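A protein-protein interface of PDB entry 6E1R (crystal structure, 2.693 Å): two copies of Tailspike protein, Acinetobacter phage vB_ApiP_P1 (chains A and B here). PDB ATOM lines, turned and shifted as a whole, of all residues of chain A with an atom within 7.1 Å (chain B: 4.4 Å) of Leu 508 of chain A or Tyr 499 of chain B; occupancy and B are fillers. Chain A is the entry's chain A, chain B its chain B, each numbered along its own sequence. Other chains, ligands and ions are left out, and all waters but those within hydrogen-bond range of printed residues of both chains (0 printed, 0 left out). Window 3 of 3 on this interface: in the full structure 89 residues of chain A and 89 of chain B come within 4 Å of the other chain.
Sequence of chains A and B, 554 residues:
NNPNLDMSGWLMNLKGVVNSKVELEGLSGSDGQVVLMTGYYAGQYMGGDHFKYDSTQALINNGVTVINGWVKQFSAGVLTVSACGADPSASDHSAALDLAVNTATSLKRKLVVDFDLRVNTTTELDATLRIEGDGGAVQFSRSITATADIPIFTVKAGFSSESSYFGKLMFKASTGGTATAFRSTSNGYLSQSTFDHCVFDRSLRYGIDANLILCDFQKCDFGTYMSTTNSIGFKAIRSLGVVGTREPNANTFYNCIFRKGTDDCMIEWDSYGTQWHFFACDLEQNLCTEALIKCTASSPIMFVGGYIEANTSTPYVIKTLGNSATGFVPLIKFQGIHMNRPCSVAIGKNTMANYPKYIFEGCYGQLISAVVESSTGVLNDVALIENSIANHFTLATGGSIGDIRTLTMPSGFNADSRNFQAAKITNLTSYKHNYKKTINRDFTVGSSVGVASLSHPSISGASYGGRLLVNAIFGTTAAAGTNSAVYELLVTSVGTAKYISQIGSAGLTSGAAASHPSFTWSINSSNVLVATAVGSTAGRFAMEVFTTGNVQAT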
ATOM      1  N   ALA A 472      18.966 -12.453   3.271  1.00  0.00           N
ATOM      2  CA  ALA A 472      19.417 -13.836   3.287  1.00  0.00           C
ATOM      3  C   ALA A 472      18.384 -14.712   2.595  1.00  0.00           C
ATOM      4  O   ALA A 472      17.178 -14.552   2.805  1.00  0.00           O
ATOM      5  CB  ALA A 472      19.648 -14.323   4.718  1.00  0.00           C
ATOM      6  N   THR A 482      11.713 -18.530  -3.584  1.00  0.00           N
ATOM      7  CA  THR A 482      12.872 -18.737  -2.726  1.00  0.00           C
ATOM      8  C   THR A 482      12.606 -18.154  -1.343  1.00  0.00           C
ATOM      9  O   THR A 482      12.151 -17.012  -1.220  1.00  0.00           O
ATOM     10  CB  THR A 482      14.116 -18.094  -3.340  1.00  0.00           C
ATOM     11  OG1 THR A 482      14.439 -18.753  -4.571  1.00  0.00           O
ATOM     12  CG2 THR A 482      15.301 -18.200  -2.390  1.00  0.00           C
ATOM     13  N   ASN A 483      12.882 -18.942  -0.306  1.00  0.00           N
ATOM     14  CA  ASN A 483      12.742 -18.455   1.060  1.00  0.00           C
ATOM     15  C   ASN A 483      13.677 -17.276   1.291  1.00  0.00           C
ATOM     16  O   ASN A 483      14.886 -17.372   1.061  1.00  0.00           O
ATOM     17  CB  ASN A 483      13.041 -19.574   2.057  1.00  0.00           C
ATOM     18  CG  ASN A 483      12.011 -20.684   2.015  1.00  0.00           C
ATOM     19  OD1 ASN A 483      10.883 -20.483   1.564  1.00  0.00           O
ATOM     20  ND2 ASN A 483      12.393 -21.862   2.491  1.00  0.00           N
ATOM     21  N   SER A 484      13.113 -16.158   1.744  1.00  0.00           N
ATOM     22  CA  SER A 484      13.853 -14.912   1.867  1.00  0.00           C
ATOM     23  C   SER A 484      13.585 -14.271   3.220  1.00  0.00           C
ATOM     24  O   SER A 484      12.531 -14.474   3.829  1.00  0.00           O
ATOM     25  CB  SER A 484      13.485 -13.931   0.743  1.00  0.00           C
ATOM     26  OG  SER A 484      14.103 -12.671   0.941  1.00  0.00           O
ATOM     27  N   ALA A 485      14.561 -13.494   3.685  1.00  0.00           N
ATOM     28  CA  ALA A 485      14.434 -12.734   4.919  1.00  0.00           C
ATOM     29  C   ALA A 485      15.326 -11.507   4.826  1.00  0.00           C
ATOM     30  O   ALA A 485      16.429 -11.574   4.277  1.00  0.00           O
ATOM     31  CB  ALA A 485      14.810 -13.575   6.143  1.00  0.00           C
ATOM     32  N   VAL A 486      14.845 -10.389   5.363  1.00  0.00           N
ATOM     33  CA  VAL A 486      15.569  -9.126   5.340  1.00  0.00           C
ATOM     34  C   VAL A 486      15.821  -8.687   6.775  1.00  0.00           C
ATOM     35  O   VAL A 486      14.977  -8.889   7.655  1.00  0.00           O
ATOM     36  CB  VAL A 486      14.813  -8.036   4.550  1.00  0.00           C
ATOM     37  CG1 VAL A 486      14.683  -8.441   3.095  1.00  0.00           C
ATOM     38  CG2 VAL A 486      13.445  -7.780   5.156  1.00  0.00           C
ATOM     39  N   TYR A 487      16.994  -8.105   7.012  1.00  0.00           N
ATOM     40  CA  TYR A 487      17.393  -7.648   8.333  1.00  0.00           C
ATOM     41  C   TYR A 487      17.967  -6.244   8.224  1.00  0.00           C
ATOM     42  O   TYR A 487      18.724  -5.945   7.296  1.00  0.00           O
ATOM     43  CB  TYR A 487      18.430  -8.590   8.959  1.00  0.00           C
ATOM     44  CG  TYR A 487      17.997 -10.039   9.018  1.00  0.00           C
ATOM     45  CD1 TYR A 487      18.165 -10.877   7.921  1.00  0.00           C
ATOM     46  CD2 TYR A 487      17.432 -10.573  10.168  1.00  0.00           C
ATOM     47  CE1 TYR A 487      17.775 -12.201   7.966  1.00  0.00           C
ATOM     48  CE2 TYR A 487      17.040 -11.899  10.222  1.00  0.00           C
ATOM     49  CZ  TYR A 487      17.215 -12.707   9.117  1.00  0.00           C
ATOM     50  OH  TYR A 487      16.828 -14.026   9.161  1.00  0.00           O
ATOM     51  N   ALA A 506      12.007  -8.919   8.501  1.00  0.00           N
ATOM     52  CA  ALA A 506      10.804  -9.348   7.804  1.00  0.00           C
ATOM     53  C   ALA A 506      11.103 -10.642   7.064  1.00  0.00           C
ATOM     54  O   ALA A 506      12.239 -10.885   6.644  1.00  0.00           O
ATOM     55  CB  ALA A 506      10.297  -8.277   6.831  1.00  0.00           C
ATOM     56  N   GLY A 507      10.076 -11.467   6.911  1.00  0.00           N
ATOM     57  CA  GLY A 507      10.208 -12.738   6.232  1.00  0.00           C
ATOM     58  C   GLY A 507      10.343 -13.905   7.190  1.00  0.00           C
ATOM     59  O   GLY A 507       9.945 -13.854   8.356  1.00  0.00           O
ATOM     60  N   LEU A 508      10.921 -14.988   6.667  1.00  0.00           N
ATOM     61  CA  LEU A 508      11.092 -16.227   7.427  1.00  0.00           C
ATOM     62  C   LEU A 508      12.301 -16.072   8.347  1.00  0.00           C
ATOM     63  O   LEU A 508      13.422 -16.483   8.041  1.00  0.00           O
ATOM     64  CB  LEU A 508      11.240 -17.414   6.485  1.00  0.00           C
ATOM     65  CG  LEU A 508      10.156 -17.520   5.410  1.00  0.00           C
ATOM     66  CD1 LEU A 508      10.426 -18.691   4.480  1.00  0.00           C
ATOM     67  CD2 LEU A 508       8.778 -17.636   6.040  1.00  0.00           C
ATOM     68  N   THR A 509      12.054 -15.470   9.510  1.00  0.00           N
ATOM     69  CA  THR A 509      13.104 -15.108  10.452  1.00  0.00           C
ATOM     70  C   THR A 509      13.066 -15.933  11.733  1.00  0.00           C
ATOM     71  O   THR A 509      13.810 -15.631  12.673  1.00  0.00           O
ATOM     72  CB  THR A 509      13.019 -13.618  10.794  1.00  0.00           C
ATOM     73  OG1 THR A 509      11.716 -13.316  11.308  1.00  0.00           O
ATOM     74  CG2 THR A 509      13.278 -12.770   9.558  1.00  0.00           C
ATOM     75  N   SER A 510      12.225 -16.965  11.799  1.00  0.00           N
ATOM     76  CA  SER A 510      12.036 -17.720  13.030  1.00  0.00           C
ATOM     77  C   SER A 510      12.572 -19.142  12.968  1.00  0.00           C
ATOM     78  O   SER A 510      12.651 -19.798  14.012  1.00  0.00           O
ATOM     79  CB  SER A 510      10.546 -17.760  13.400  1.00  0.00           C
ATOM     80  OG  SER A 510      10.059 -16.461  13.684  1.00  0.00           O
ATOM     81  N   GLY A 511      12.938 -19.636  11.790  1.00  0.00           N
ATOM     82  CA  GLY A 511      13.502 -20.969  11.692  1.00  0.00           C
ATOM     83  C   GLY A 511      12.501 -22.085  11.879  1.00  0.00           C
ATOM     84  O   GLY A 511      12.856 -23.144  12.404  1.00  0.00           O
ATOM     85  N   ALA A 512      11.250 -21.875  11.462  1.00  0.00           N
ATOM     86  CA  ALA A 512      10.238 -22.918  11.594  1.00  0.00           C
ATOM     87  C   ALA A 512      10.592 -24.146  10.767  1.00  0.00           C
ATOM     88  O   ALA A 512      10.166 -25.259  11.095  1.00  0.00           O
ATOM     89  CB  ALA A 512       8.868 -22.377  11.188  1.00  0.00           C
ATOM     90  N   SER A 515      14.925 -24.826   5.755  1.00  0.00           N
ATOM     91  CA  SER A 515      15.198 -23.999   4.585  1.00  0.00           C
ATOM     92  C   SER A 515      14.877 -22.523   4.798  1.00  0.00           C
ATOM     93  O   SER A 515      14.948 -21.748   3.838  1.00  0.00           O
ATOM     94  CB  SER A 515      14.415 -24.529   3.381  1.00  0.00           C
ATOM     95  OG  SER A 515      13.019 -24.497   3.626  1.00  0.00           O
ATOM     96  N   HIS A 516      14.529 -22.113   6.017  1.00  0.00           N
ATOM     97  CA  HIS A 516      14.198 -20.710   6.253  1.00  0.00           C
ATOM     98  C   HIS A 516      15.465 -19.919   6.558  1.00  0.00           C
ATOM     99  O   HIS A 516      16.267 -20.348   7.395  1.00  0.00           O
ATOM    100  CB  HIS A 516      13.214 -20.571   7.406  1.00  0.00           C
ATOM    101  CG  HIS A 516      11.869 -21.168   7.129  1.00  0.00           C
ATOM    102  ND1 HIS A 516      10.806 -21.042   7.997  1.00  0.00           N
ATOM    103  CD2 HIS A 516      11.413 -21.891   6.077  1.00  0.00           C
ATOM    104  CE1 HIS A 516       9.754 -21.664   7.493  1.00  0.00           C
ATOM    105  NE2 HIS A 516      10.096 -22.187   6.330  1.00  0.00           N
ATOM    106  N   PRO A 517      15.680 -18.773   5.908  1.00  0.00           N
ATOM    107  CA  PRO A 517      16.900 -17.971   6.151  1.00  0.00           C
ATOM    108  C   PRO A 517      16.807 -17.141   7.427  1.00  0.00           C
ATOM    109  O   PRO A 517      16.779 -15.905   7.419  1.00  0.00           O
ATOM    110  CB  PRO A 517      16.978 -17.108   4.889  1.00  0.00           C
ATOM    111  CG  PRO A 517      15.550 -16.908   4.505  1.00  0.00           C
ATOM    112  CD  PRO A 517      14.834 -18.187   4.855  1.00  0.00           C
ATOM    113  N   SER A 518      16.770 -17.833   8.563  1.00  0.00           N
ATOM    114  CA  SER A 518      16.575 -17.208   9.866  1.00  0.00           C
ATOM    115  C   SER A 518      17.906 -17.159  10.607  1.00  0.00           C
ATOM    116  O   SER A 518      18.505 -18.206  10.881  1.00  0.00           O
ATOM    117  CB  SER A 518      15.535 -17.975  10.677  1.00  0.00           C
ATOM    118  OG  SER A 518      14.366 -18.204   9.909  1.00  0.00           O
ATOM    119  N   PHE A 519      18.362 -15.952  10.938  1.00  0.00           N
ATOM    120  CA  PHE A 519      19.678 -15.790  11.541  1.00  0.00           C
ATOM    121  C   PHE A 519      19.661 -14.645  12.544  1.00  0.00           C
ATOM    122  O   PHE A 519      18.924 -13.667  12.387  1.00  0.00           O
ATOM    123  CB  PHE A 519      20.752 -15.537  10.475  1.00  0.00           C
ATOM    124  CG  PHE A 519      20.770 -16.566   9.383  1.00  0.00           C
ATOM    125  CD1 PHE A 519      21.373 -17.796   9.582  1.00  0.00           C
ATOM    126  CD2 PHE A 519      20.169 -16.309   8.163  1.00  0.00           C
ATOM    127  CE1 PHE A 519      21.383 -18.748   8.581  1.00  0.00           C
ATOM    128  CE2 PHE A 519      20.177 -17.255   7.159  1.00  0.00           C
ATOM    129  CZ  PHE A 519      20.786 -18.477   7.368  1.00  0.00           C
ATOM    130  N   THR A 537      16.879 -23.904  11.316  1.00  0.00           N
ATOM    131  CA  THR A 537      17.573 -23.480  10.107  1.00  0.00           C
ATOM    132  C   THR A 537      18.875 -24.250   9.926  1.00  0.00           C
ATOM    133  O   THR A 537      19.719 -24.293  10.826  1.00  0.00           O
ATOM    134  CB  THR A 537      17.853 -21.977  10.161  1.00  0.00           C
ATOM    135  OG1 THR A 537      16.617 -21.255  10.078  1.00  0.00           O
ATOM    136  CG2 THR A 537      18.767 -21.556   9.017  1.00  0.00           C
ATOM    137  N   LEU B 490      10.197  -2.502   5.794  1.00  0.00           N
ATOM    138  CA  LEU B 490      10.967  -3.653   5.336  1.00  0.00           C
ATOM    139  C   LEU B 490      10.035  -4.614   4.610  1.00  0.00           C
ATOM    140  O   LEU B 490       9.005  -5.015   5.159  1.00  0.00           O
ATOM    141  CB  LEU B 490      11.647  -4.368   6.505  1.00  0.00           C
ATOM    142  CG  LEU B 490      12.977  -3.804   7.003  1.00  0.00           C
ATOM    143  CD1 LEU B 490      13.571  -4.713   8.068  1.00  0.00           C
ATOM    144  CD2 LEU B 490      13.948  -3.623   5.847  1.00  0.00           C
ATOM    145  N   VAL B 491      10.398  -4.983   3.382  1.00  0.00           N
ATOM    146  CA  VAL B 491       9.557  -5.836   2.554  1.00  0.00           C
ATOM    147  C   VAL B 491      10.375  -6.997   2.007  1.00  0.00           C
ATOM    148  O   VAL B 491      11.584  -6.883   1.779  1.00  0.00           O
ATOM    149  CB  VAL B 491       8.898  -5.051   1.395  1.00  0.00           C
ATOM    150  CG1 VAL B 491       7.961  -3.984   1.937  1.00  0.00           C
ATOM    151  CG2 VAL B 491       9.958  -4.435   0.492  1.00  0.00           C
ATOM    152  N   THR B 492       9.700  -8.126   1.813  1.00  0.00           N
ATOM    153  CA  THR B 492      10.245  -9.301   1.144  1.00  0.00           C
ATOM    154  C   THR B 492       9.082 -10.231   0.835  1.00  0.00           C
ATOM    155  O   THR B 492       7.998 -10.102   1.412  1.00  0.00           O
ATOM    156  CB  THR B 492      11.302 -10.019   1.993  1.00  0.00           C
ATOM    157  OG1 THR B 492      11.872 -11.093   1.234  1.00  0.00           O
ATOM    158  CG2 THR B 492      10.681 -10.578   3.262  1.00  0.00           C
ATOM    159  N   SER B 493       9.313 -11.167  -0.083  1.00  0.00           N
ATOM    160  CA  SER B 493       8.260 -12.074  -0.516  1.00  0.00           C
ATOM    161  C   SER B 493       8.811 -13.481  -0.685  1.00  0.00           C
ATOM    162  O   SER B 493       9.987 -13.672  -1.004  1.00  0.00           O
ATOM    163  CB  SER B 493       7.626 -11.609  -1.836  1.00  0.00           C
ATOM    164  OG  SER B 493       8.562 -11.666  -2.898  1.00  0.00           O
ATOM    165  N   VAL B 494       7.944 -14.466  -0.453  1.00  0.00           N
ATOM    166  CA  VAL B 494       8.248 -15.869  -0.721  1.00  0.00           C
ATOM    167  C   VAL B 494       7.039 -16.482  -1.415  1.00  0.00           C
ATOM    168  O   VAL B 494       6.108 -16.961  -0.757  1.00  0.00           O
ATOM    169  CB  VAL B 494       8.601 -16.645   0.562  1.00  0.00           C
ATOM    170  CG1 VAL B 494       8.952 -18.088   0.225  1.00  0.00           C
ATOM    171  CG2 VAL B 494       9.749 -15.981   1.308  1.00  0.00           C
ATOM    172  N   ALA B 497       3.326 -15.494  -0.467  1.00  0.00           N
ATOM    173  CA  ALA B 497       3.406 -14.879   0.849  1.00  0.00           C
ATOM    174  C   ALA B 497       4.127 -13.540   0.761  1.00  0.00           C
ATOM    175  O   ALA B 497       5.248 -13.458   0.250  1.00  0.00           O
ATOM    176  CB  ALA B 497       4.125 -15.806   1.828  1.00  0.00           C
ATOM    177  N   LYS B 498       3.477 -12.491   1.258  1.00  0.00           N
ATOM    178  CA  LYS B 498       4.028 -11.143   1.257  1.00  0.00           C
ATOM    179  C   LYS B 498       4.354 -10.745   2.690  1.00  0.00           C
ATOM    180  O   LYS B 498       3.528 -10.926   3.591  1.00  0.00           O
ATOM    181  CB  LYS B 498       3.046 -10.146   0.639  1.00  0.00           C
ATOM    182  CG  LYS B 498       2.421 -10.608  -0.671  1.00  0.00           C
ATOM    183  CD  LYS B 498       3.468 -11.052  -1.682  1.00  0.00           C
ATOM    184  CE  LYS B 498       2.811 -11.605  -2.936  1.00  0.00           C
ATOM    185  NZ  LYS B 498       3.802 -12.177  -3.889  1.00  0.00           N
ATOM    186  N   TYR B 499       5.550 -10.203   2.896  1.00  0.00           N
ATOM    187  CA  TYR B 499       6.025  -9.831   4.223  1.00  0.00           C
ATOM    188  C   TYR B 499       6.392  -8.356   4.219  1.00  0.00           C
ATOM    189  O   TYR B 499       7.272  -7.933   3.463  1.00  0.00           O
ATOM    190  CB  TYR B 499       7.230 -10.682   4.633  1.00  0.00           C
ATOM    191  CG  TYR B 499       6.949 -12.167   4.636  1.00  0.00           C
ATOM    192  CD1 TYR B 499       6.525 -12.811   5.791  1.00  0.00           C
ATOM    193  CD2 TYR B 499       7.103 -12.924   3.483  1.00  0.00           C
ATOM    194  CE1 TYR B 499       6.264 -14.166   5.797  1.00  0.00           C
ATOM    195  CE2 TYR B 499       6.845 -14.279   3.479  1.00  0.00           C
ATOM    196  CZ  TYR B 499       6.426 -14.897   4.638  1.00  0.00           C
ATOM    197  OH  TYR B 499       6.167 -16.249   4.637  1.00  0.00           O
ATOM    198  N   ILE B 500       5.717  -7.578   5.060  1.00  0.00           N
ATOM    199  CA  ILE B 500       6.005  -6.158   5.212  1.00  0.00           C
ATOM    200  C   ILE B 500       5.995  -5.829   6.699  1.00  0.00           C
ATOM    201  O   ILE B 500       5.146  -6.317   7.452  1.00  0.00           O
ATOM    202  CB  ILE B 500       5.007  -5.279   4.427  1.00  0.00           C
ATOM    203  CG1 ILE B 500       5.363  -3.797   4.573  1.00  0.00           C
ATOM    204  CG2 ILE B 500       3.570  -5.549   4.867  1.00  0.00           C
ATOM    205  CD1 ILE B 500       4.552  -2.885   3.681  1.00  0.00           C
ATOM    206  N   ILE B 523       1.021  -5.442   1.273  1.00  0.00           N
ATOM    207  CA  ILE B 523       1.374  -5.951  -0.047  1.00  0.00           C
ATOM    208  C   ILE B 523       0.321  -6.978  -0.438  1.00  0.00           C
ATOM    209  O   ILE B 523       0.110  -7.960   0.284  1.00  0.00           O
ATOM    210  CB  ILE B 523       2.778  -6.582  -0.069  1.00  0.00           C
ATOM    211  CG1 ILE B 523       3.825  -5.590   0.445  1.00  0.00           C
ATOM    212  CG2 ILE B 523       3.129  -7.046  -1.476  1.00  0.00           C
ATOM    213  CD1 ILE B 523       5.220  -6.173   0.547  1.00  0.00           C
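No position is printed for both chains.
Of the 13 pairs that touch across the chains among the printed residues, none has its exchanged pair printed and touching as well.
Hydrophobic or aromatic side chains of chain A within 4 Å of the printed part of chain B: Val 486, Ala 506 and Leu 508.
Along chain A the printed residues that touch a printed residue of chain B span positions 482 to 508.
Of the 10 printed residues of chain B, 6 touch a printed residue of chain A.
Printed residues of chain B that touch a printed residue of chain A: Leu 490, Val 491, Thr 492, Ser 493, Val 494 and Tyr 499.
Among the printed residues, 13 pairs touch across the chains.
Among the printed residues, no Asp or Glu carboxylate lies within 4 Å of a Lys or Arg side-chain nitrogen of the other chain.
Thr 482 of chain A touches Ser 493 of chain B.
Thr 482 of chain A touches Val 494 of chain B.
CB of Ser 484 of chain A touches O of Ser 493 of chain B, 3.9 Å away.
CG2 of Val 494 of chain B touches N of Ser 484 of chain A, at 3.4 Å.
CG1 of Val 486 of chain A touches O of Val 491 of chain B, 3.7 Å away.
Val 486 of chain A touches Thr 492 of chain B.
Leu 490 of chain B touches Ala 506 of chain A (O to CB, 3.9 Å).
Thr 492 of chain B touches Ala 506 of chain A.
Gly 507 of chain A touches Thr 492 of chain B.
Leu 508 of chain A touches Tyr 499 of chain B (CD2 to OH, 3.3 Å).
The backbone carbonyl oxygen of Ser 484 of chain A sits at hydrogen-bond distance from the backbone NH of Leu 508 of chain A.
N of Tyr 499 of chain B lies within hydrogen-bond range of O of Thr 492 of chain B, 2.9 Å away.
O of Gly 507 of chain A lies within hydrogen-bond range of OG1 of Thr 509 of chain A.
O of Leu 508 of chain A lies within hydrogen-bond range of OG of Ser 518 of chain A, at 2.7 Å.
O of Ala 506 of chain A lies within hydrogen-bond range of N of Val 486 of chain A (2.9 Å).
The backbone carbonyl oxygen (O) of Ser 515 of chain A is in hydrogen-bond range of the side-chain amide nitrogen (ND2) of Asn 483 of chain A (2.9 Å).
OG of Ser 484 of chain A sits at hydrogen-bond distance from OG1 of Thr 492 of chain B, at 2.7 Å.
Leu 508 of chain A touches just one residue of chain B: Tyr 499 (3.3 Å).
Of the printed residues of chain A, Tyr 499 of chain B touches Gly 507 (3.7 Å) and Leu 508 (3.3 Å).
Printed residues of chain B within 4 Å of Gly 507 of chain A: Thr 492 and Tyr 499.
Printed residues of chain A within 4 Å of Thr 492 of chain B: Ser 484 (2.7 Å), Val 486 (3.9 Å), Ala 506 (3.7 Å) and Gly 507 (3.7 Å).
Printed residues of chain B within 4 Å of Asn 483 of chain A: Val 494 (3.4 Å).
Of the printed residues of chain A, Val 491 of chain B touches Val 486 (3.7 Å).
Printed residues of chain A within 4 Å of Val 494 of chain B: Thr 482, Asn 483 and Ser 484.
Lys 498 of chain B touches none of the printed residues of chain A.
Thr 509 of chain A touches none of the printed residues of chain B.
The nearest residue of chain A that does not touch Tyr 499 of chain B is Ala 506 of chain A (4.5 Å).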
